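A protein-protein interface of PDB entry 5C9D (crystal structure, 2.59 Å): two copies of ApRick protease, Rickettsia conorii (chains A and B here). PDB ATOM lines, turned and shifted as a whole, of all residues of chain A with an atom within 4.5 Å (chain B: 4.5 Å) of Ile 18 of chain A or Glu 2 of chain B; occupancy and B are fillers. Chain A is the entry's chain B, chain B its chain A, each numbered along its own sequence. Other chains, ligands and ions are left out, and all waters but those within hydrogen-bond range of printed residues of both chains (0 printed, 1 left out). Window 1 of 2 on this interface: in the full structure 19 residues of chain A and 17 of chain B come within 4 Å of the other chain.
O of Tyr 17 of chain A sits close to SD of Met 1 of chain B (3.1 Å).
N of Val 3 of chain B lies within hydrogen-bond range of O of Ile 7 of chain A, at 3.1 Å.
The backbone carbonyl oxygen of Glu 2 of chain B sits at hydrogen-bond distance from the backbone NH of Ala 125 of chain B (2.5 Å).
O of Ile 18 of chain A lies within hydrogen-bond range of N of Phe 29 of chain A (2.9 Å).
N of Val 31 of chain A sits at hydrogen-bond distance from O of Phe 16 of chain A (3.1 Å).
The backbone carbonyl oxygen of Gly 4 of chain B sits at hydrogen-bond distance from the backbone NH of Tyr 123 of chain B, 3.0 Å away.
OH of Tyr 123 of chain B sits at hydrogen-bond distance from OE2 of Glu 2 of chain B (2.8 Å).
Among the printed residues, merely in contact across the chains: Ile 6 of chain A with Glu 2 of chain B (3.9 Å), Ile 6 of chain A with Val 3 of chain B (3.7 Å), Ile 6 of chain A with Gly 4 of chain B (3.6 Å), Ile 6 of chain A with Tyr 123 of chain B (3.5 Å), Ile 7 of chain A with Met 1 of chain B (3.8 Å), Ile 7 of chain A with Glu 2 of chain B (3.2 Å), Ile 8 of chain A with Met 1 of chain B (3.6 Å), Phe 16 of chain A with Met 1 of chain B (2.9 Å), Ile 18 of chain A with Glu 2 of chain B (3.3 Å), Asn 19 of chain A with Met 1 of chain B (3.6 Å), Ile 80 of chain A with Glu 2 of chain B (3.6 Å) and Ile 80 of chain A with Tyr 123 of chain B (3.8 Å).
Printed residues of chain B within 4 Å of Ile 7 of chain A: Met 1, Glu 2 and Val 3.
Printed residues of chain B within 4 Å of Ile 8 of chain A: Met 1 (3.6 Å).
Of the printed residues of chain B, Tyr 17 of chain A touches Met 1 (2.8 Å).
Ile 27 of chain A touches none of the printed residues of chain B.
Of the printed residues of chain B, Ile 80 of chain A touches Glu 2 and Tyr 123.
Glu 2 of chain B touches four residues of chain A.
Of the printed residues of chain A, Tyr 123 of chain B touches Ile 6 (3.5 Å) and Ile 80 (3.8 Å).
Ala 124 of chain B touches none of the printed residues of chain A.
The nearest residue of chain B that does not touch Ile 18 of chain A is Met 1 of chain B (4.4 Å).
The nearest printed residue of chain B that does not touch Ile 80 of chain A is Ala 125 of chain B (7.2 Å).
Hydrophobic or aromatic side chains of chain B within 4 Å of the printed part of chain A: Met 1 and Tyr 123.
Of the 14 printed residues of chain A, 8 touch a printed residue of chain B.
Hydrophobic or aromatic side chains of chain A within 4 Å of the printed part of chain B: Ile 6, Ile 7, Phe 16, Ile 18 and Ile 80.
Among the printed residues, 14 pairs touch across the chains.
Among the printed residues, no Asp or Glu carboxylate lies within 4 Å of a Lys or Arg side-chain nitrogen of the other chain.
No position is printed for both chains.
Of the 14 pairs that touch across the chains among the printed residues, none has its exchanged pair printed and touching as well.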
ATOM      1  N   ILE A   6     -24.816 -32.849   8.015  1.00  0.00           N
ATOM      2  CA  ILE A   6     -25.050 -31.826   9.034  1.00  0.00           C
ATOM      3  C   ILE A   6     -26.542 -31.485   9.102  1.00  0.00           C
ATOM      4  O   ILE A   6     -27.144 -31.161   8.092  1.00  0.00           O
ATOM      5  CB  ILE A   6     -24.240 -30.539   8.747  1.00  0.00           C
ATOM      6  CG1 ILE A   6     -22.770 -30.862   8.399  1.00  0.00           C
ATOM      7  CG2 ILE A   6     -24.325 -29.564   9.922  1.00  0.00           C
ATOM      8  CD1 ILE A   6     -21.997 -31.614   9.472  1.00  0.00           C
ATOM      9  N   ILE A   7     -27.123 -31.552  10.294  1.00  0.00           N
ATOM     10  CA  ILE A   7     -28.518 -31.223  10.504  1.00  0.00           C
ATOM     11  C   ILE A   7     -28.709 -30.066  11.481  1.00  0.00           C
ATOM     12  O   ILE A   7     -28.108 -30.073  12.546  1.00  0.00           O
ATOM     13  CB  ILE A   7     -29.251 -32.434  11.076  1.00  0.00           C
ATOM     14  CG1 ILE A   7     -28.848 -33.684  10.279  1.00  0.00           C
ATOM     15  CG2 ILE A   7     -30.758 -32.168  11.068  1.00  0.00           C
ATOM     16  CD1 ILE A   7     -29.291 -34.991  10.898  1.00  0.00           C
ATOM     17  N   ILE A   8     -29.600 -29.120  11.154  1.00  0.00           N
ATOM     18  CA  ILE A   8     -29.629 -27.813  11.827  1.00  0.00           C
ATOM     19  C   ILE A   8     -31.021 -27.370  12.310  1.00  0.00           C
ATOM     20  O   ILE A   8     -31.768 -26.701  11.604  1.00  0.00           O
ATOM     21  CB  ILE A   8     -29.016 -26.745  10.898  1.00  0.00           C
ATOM     22  CG1 ILE A   8     -27.666 -27.229  10.347  1.00  0.00           C
ATOM     23  CG2 ILE A   8     -28.843 -25.430  11.635  1.00  0.00           C
ATOM     24  CD1 ILE A   8     -26.962 -26.240   9.443  1.00  0.00           C
ATOM     25  N   PHE A  16     -31.720 -20.823  10.834  1.00  0.00           N
ATOM     26  CA  PHE A  16     -30.753 -21.345  11.788  1.00  0.00           C
ATOM     27  C   PHE A  16     -29.302 -21.126  11.416  1.00  0.00           C
ATOM     28  O   PHE A  16     -28.951 -20.778  10.282  1.00  0.00           O
ATOM     29  CB  PHE A  16     -31.006 -22.806  12.183  1.00  0.00           C
ATOM     30  CG  PHE A  16     -30.735 -23.114  13.663  1.00  0.00           C
ATOM     31  CD1 PHE A  16     -30.629 -22.102  14.610  1.00  0.00           C
ATOM     32  CD2 PHE A  16     -30.618 -24.412  14.111  1.00  0.00           C
ATOM     33  CE1 PHE A  16     -30.398 -22.367  15.947  1.00  0.00           C
ATOM     34  CE2 PHE A  16     -30.402 -24.688  15.456  1.00  0.00           C
ATOM     35  CZ  PHE A  16     -30.297 -23.659  16.377  1.00  0.00           C
ATOM     36  N   TYR A  17     -28.485 -21.350  12.437  1.00  0.00           N
ATOM     37  CA  TYR A  17     -27.167 -20.816  12.554  1.00  0.00           C
ATOM     38  C   TYR A  17     -26.239 -21.970  12.878  1.00  0.00           C
ATOM     39  O   TYR A  17     -26.569 -22.823  13.695  1.00  0.00           O
ATOM     40  CB  TYR A  17     -27.146 -19.781  13.689  1.00  0.00           C
ATOM     41  CG  TYR A  17     -28.288 -18.780  13.613  1.00  0.00           C
ATOM     42  CD1 TYR A  17     -28.219 -17.685  12.783  1.00  0.00           C
ATOM     43  CD2 TYR A  17     -29.431 -18.951  14.361  1.00  0.00           C
ATOM     44  CE1 TYR A  17     -29.251 -16.780  12.706  1.00  0.00           C
ATOM     45  CE2 TYR A  17     -30.482 -18.064  14.287  1.00  0.00           C
ATOM     46  CZ  TYR A  17     -30.389 -16.979  13.450  1.00  0.00           C
ATOM     47  OH  TYR A  17     -31.421 -16.075  13.368  1.00  0.00           O
ATOM     48  N   ILE A  18     -25.100 -22.005  12.203  1.00  0.00           N
ATOM     49  CA  ILE A  18     -24.050 -22.945  12.531  1.00  0.00           C
ATOM     50  C   ILE A  18     -22.976 -22.110  13.189  1.00  0.00           C
ATOM     51  O   ILE A  18     -22.983 -20.878  13.089  1.00  0.00           O
ATOM     52  CB  ILE A  18     -23.427 -23.633  11.299  1.00  0.00           C
ATOM     53  CG1 ILE A  18     -24.353 -23.540  10.094  1.00  0.00           C
ATOM     54  CG2 ILE A  18     -23.095 -25.084  11.614  1.00  0.00           C
ATOM     55  CD1 ILE A  18     -23.956 -24.424   8.935  1.00  0.00           C
ATOM     56  N   ASN A  19     -22.068 -22.790  13.878  1.00  0.00           N
ATOM     57  CA  ASN A  19     -20.837 -22.194  14.335  1.00  0.00           C
ATOM     58  C   ASN A  19     -19.707 -22.812  13.541  1.00  0.00           C
ATOM     59  O   ASN A  19     -19.621 -24.042  13.401  1.00  0.00           O
ATOM     60  CB  ASN A  19     -20.649 -22.435  15.814  1.00  0.00           C
ATOM     61  CG  ASN A  19     -21.755 -21.823  16.651  1.00  0.00           C
ATOM     62  OD1 ASN A  19     -21.762 -20.614  16.854  1.00  0.00           O
ATOM     63  ND2 ASN A  19     -22.677 -22.657  17.172  1.00  0.00           N
ATOM     64  N   ALA A  20     -18.892 -21.941  12.965  1.00  0.00           N
ATOM     65  CA  ALA A  20     -17.702 -22.344  12.275  1.00  0.00           C
ATOM     66  C   ALA A  20     -16.555 -21.655  12.975  1.00  0.00           C
ATOM     67  O   ALA A  20     -16.740 -20.673  13.691  1.00  0.00           O
ATOM     68  CB  ALA A  20     -17.764 -21.936  10.826  1.00  0.00           C
ATOM     69  N   ILE A  27     -17.043 -18.180  14.897  1.00  0.00           N
ATOM     70  CA  ILE A  27     -17.986 -17.212  14.415  1.00  0.00           C
ATOM     71  C   ILE A  27     -19.319 -17.947  14.290  1.00  0.00           C
ATOM     72  O   ILE A  27     -19.356 -19.156  13.973  1.00  0.00           O
ATOM     73  CB  ILE A  27     -17.529 -16.631  13.067  1.00  0.00           C
ATOM     74  CG1 ILE A  27     -16.235 -15.837  13.259  1.00  0.00           C
ATOM     75  CG2 ILE A  27     -18.626 -15.782  12.435  1.00  0.00           C
ATOM     76  CD1 ILE A  27     -16.288 -14.915  14.449  1.00  0.00           C
ATOM     77  N   LYS A  28     -20.393 -17.207  14.575  1.00  0.00           N
ATOM     78  CA  LYS A  28     -21.762 -17.700  14.496  1.00  0.00           C
ATOM     79  C   LYS A  28     -22.405 -17.183  13.196  1.00  0.00           C
ATOM     80  O   LYS A  28     -22.484 -15.978  12.943  1.00  0.00           O
ATOM     81  CB  LYS A  28     -22.542 -17.274  15.744  1.00  0.00           C
ATOM     82  CG  LYS A  28     -21.755 -17.509  17.039  1.00  0.00           C
ATOM     83  CD  LYS A  28     -22.642 -17.962  18.190  1.00  0.00           C
ATOM     84  CE  LYS A  28     -21.829 -18.506  19.358  1.00  0.00           C
ATOM     85  NZ  LYS A  28     -22.705 -19.089  20.418  1.00  0.00           N
ATOM     86  N   PHE A  29     -22.848 -18.121  12.370  1.00  0.00           N
ATOM     87  CA  PHE A  29     -23.201 -17.844  11.000  1.00  0.00           C
ATOM     88  C   PHE A  29     -24.659 -18.169  10.733  1.00  0.00           C
ATOM     89  O   PHE A  29     -25.116 -19.284  11.030  1.00  0.00           O
ATOM     90  CB  PHE A  29     -22.375 -18.742  10.102  1.00  0.00           C
ATOM     91  CG  PHE A  29     -21.015 -18.210   9.780  1.00  0.00           C
ATOM     92  CD1 PHE A  29     -20.867 -17.008   9.078  1.00  0.00           C
ATOM     93  CD2 PHE A  29     -19.879 -18.937  10.117  1.00  0.00           C
ATOM     94  CE1 PHE A  29     -19.606 -16.532   8.739  1.00  0.00           C
ATOM     95  CE2 PHE A  29     -18.616 -18.465   9.778  1.00  0.00           C
ATOM     96  CZ  PHE A  29     -18.476 -17.267   9.085  1.00  0.00           C
ATOM     97  N   VAL A  31     -27.183 -19.411   8.204  1.00  0.00           N
ATOM     98  CA  VAL A  31     -27.007 -20.231   7.019  1.00  0.00           C
ATOM     99  C   VAL A  31     -27.942 -19.659   5.970  1.00  0.00           C
ATOM    100  O   VAL A  31     -29.167 -19.649   6.161  1.00  0.00           O
ATOM    101  CB  VAL A  31     -27.330 -21.716   7.264  1.00  0.00           C
ATOM    102  CG1 VAL A  31     -26.710 -22.559   6.161  1.00  0.00           C
ATOM    103  CG2 VAL A  31     -26.797 -22.177   8.610  1.00  0.00           C
ATOM    104  N   ILE A  80     -16.070 -26.498  10.117  1.00  0.00           N
ATOM    105  CA  ILE A  80     -17.306 -26.933  10.778  1.00  0.00           C
ATOM    106  C   ILE A  80     -16.962 -28.283  11.416  1.00  0.00           C
ATOM    107  O   ILE A  80     -17.484 -28.644  12.476  1.00  0.00           O
ATOM    108  CB  ILE A  80     -18.528 -27.131   9.852  1.00  0.00           C
ATOM    109  CG1 ILE A  80     -18.541 -26.208   8.613  1.00  0.00           C
ATOM    110  CG2 ILE A  80     -19.790 -26.978  10.693  1.00  0.00           C
ATOM    111  CD1 ILE A  80     -18.978 -24.775   8.851  1.00  0.00           C
ATOM    112  N   LEU A 101     -23.223 -17.602   6.080  1.00  0.00           N
ATOM    113  CA  LEU A 101     -22.576 -18.772   5.592  1.00  0.00           C
ATOM    114  C   LEU A 101     -23.255 -19.088   4.295  1.00  0.00           C
ATOM    115  O   LEU A 101     -24.348 -19.627   4.273  1.00  0.00           O
ATOM    116  CB  LEU A 101     -22.747 -19.887   6.583  1.00  0.00           C
ATOM    117  CG  LEU A 101     -21.815 -21.051   6.348  1.00  0.00           C
ATOM    118  CD1 LEU A 101     -21.771 -21.868   7.634  1.00  0.00           C
ATOM    119  CD2 LEU A 101     -22.265 -21.858   5.131  1.00  0.00           C
ATOM    120  N   MET B   1     -29.110 -28.651  18.512  1.00  0.00           N
ATOM    121  CA  MET B   1     -28.930 -27.512  17.552  1.00  0.00           C
ATOM    122  C   MET B   1     -28.253 -27.897  16.267  1.00  0.00           C
ATOM    123  O   MET B   1     -28.635 -27.391  15.226  1.00  0.00           O
ATOM    124  CB  MET B   1     -28.089 -26.382  18.149  1.00  0.00           C
ATOM    125  CG  MET B   1     -27.953 -25.127  17.266  1.00  0.00           C
ATOM    126  SD  MET B   1     -26.651 -24.910  16.007  1.00  0.00           S
ATOM    127  CE  MET B   1     -26.100 -23.254  16.419  1.00  0.00           C
ATOM    128  N   GLU B   2     -27.199 -28.709  16.334  1.00  0.00           N
ATOM    129  CA  GLU B   2     -26.451 -29.102  15.107  1.00  0.00           C
ATOM    130  C   GLU B   2     -25.752 -30.427  15.351  1.00  0.00           C
ATOM    131  O   GLU B   2     -25.136 -30.637  16.398  1.00  0.00           O
ATOM    132  CB  GLU B   2     -25.444 -28.024  14.655  1.00  0.00           C
ATOM    133  CG  GLU B   2     -24.371 -28.451  13.626  1.00  0.00           C
ATOM    134  CD  GLU B   2     -23.046 -27.702  13.807  1.00  0.00           C
ATOM    135  OE1 GLU B   2     -23.023 -26.689  14.553  1.00  0.00           O
ATOM    136  OE2 GLU B   2     -22.000 -28.122  13.248  1.00  0.00           O
ATOM    137  N   VAL B   3     -25.837 -31.297  14.349  1.00  0.00           N
ATOM    138  CA  VAL B   3     -25.534 -32.704  14.510  1.00  0.00           C
ATOM    139  C   VAL B   3     -24.883 -33.258  13.265  1.00  0.00           C
ATOM    140  O   VAL B   3     -25.568 -33.488  12.263  1.00  0.00           O
ATOM    141  CB  VAL B   3     -26.835 -33.473  14.721  1.00  0.00           C
ATOM    142  CG1 VAL B   3     -26.588 -34.982  14.682  1.00  0.00           C
ATOM    143  CG2 VAL B   3     -27.483 -33.012  16.017  1.00  0.00           C
ATOM    144  N   GLY B   4     -23.579 -33.504  13.339  1.00  0.00           N
ATOM    145  CA  GLY B   4     -22.797 -33.912  12.169  1.00  0.00           C
ATOM    146  C   GLY B   4     -21.930 -35.163  12.281  1.00  0.00           C
ATOM    147  O   GLY B   4     -21.642 -35.657  13.382  1.00  0.00           O
ATOM    148  N   TYR B 123     -21.255 -35.670  16.356  1.00  0.00           N
ATOM    149  CA  TYR B 123     -21.239 -34.678  17.433  1.00  0.00           C
ATOM    150  C   TYR B 123     -22.550 -33.937  17.479  1.00  0.00           C
ATOM    151  O   TYR B 123     -23.320 -33.979  16.536  1.00  0.00           O
ATOM    152  CB  TYR B 123     -20.112 -33.672  17.211  1.00  0.00           C
ATOM    153  CG  TYR B 123     -20.289 -32.842  15.953  1.00  0.00           C
ATOM    154  CD1 TYR B 123     -21.005 -31.645  15.987  1.00  0.00           C
ATOM    155  CD2 TYR B 123     -19.738 -33.250  14.729  1.00  0.00           C
ATOM    156  CE1 TYR B 123     -21.166 -30.866  14.853  1.00  0.00           C
ATOM    157  CE2 TYR B 123     -19.898 -32.473  13.583  1.00  0.00           C
ATOM    158  CZ  TYR B 123     -20.621 -31.287  13.656  1.00  0.00           C
ATOM    159  OH  TYR B 123     -20.809 -30.503  12.544  1.00  0.00           O
ATOM    160  N   ALA B 124     -22.775 -33.235  18.574  1.00  0.00           N
ATOM    161  CA  ALA B 124     -23.964 -32.420  18.733  1.00  0.00           C
ATOM    162  C   ALA B 124     -23.578 -31.020  19.247  1.00  0.00           C
ATOM    163  O   ALA B 124     -23.093 -30.901  20.359  1.00  0.00           O
ATOM    164  CB  ALA B 124     -24.938 -33.116  19.685  1.00  0.00           C
ATOM    165  N   ALA B 125     -23.800 -29.971  18.457  1.00  0.00           N
ATOM    166  CA  ALA B 125     -23.307 -28.624  18.802  1.00  0.00           C
ATOM    167  C   ALA B 125     -24.419 -27.593  19.000  1.00  0.00           C
ATOM    168  O   ALA B 125     -24.899 -26.957  18.037  1.00  0.00           O
ATOM    169  CB  ALA B 125     -22.334 -28.124  17.738  1.00  0.00           C
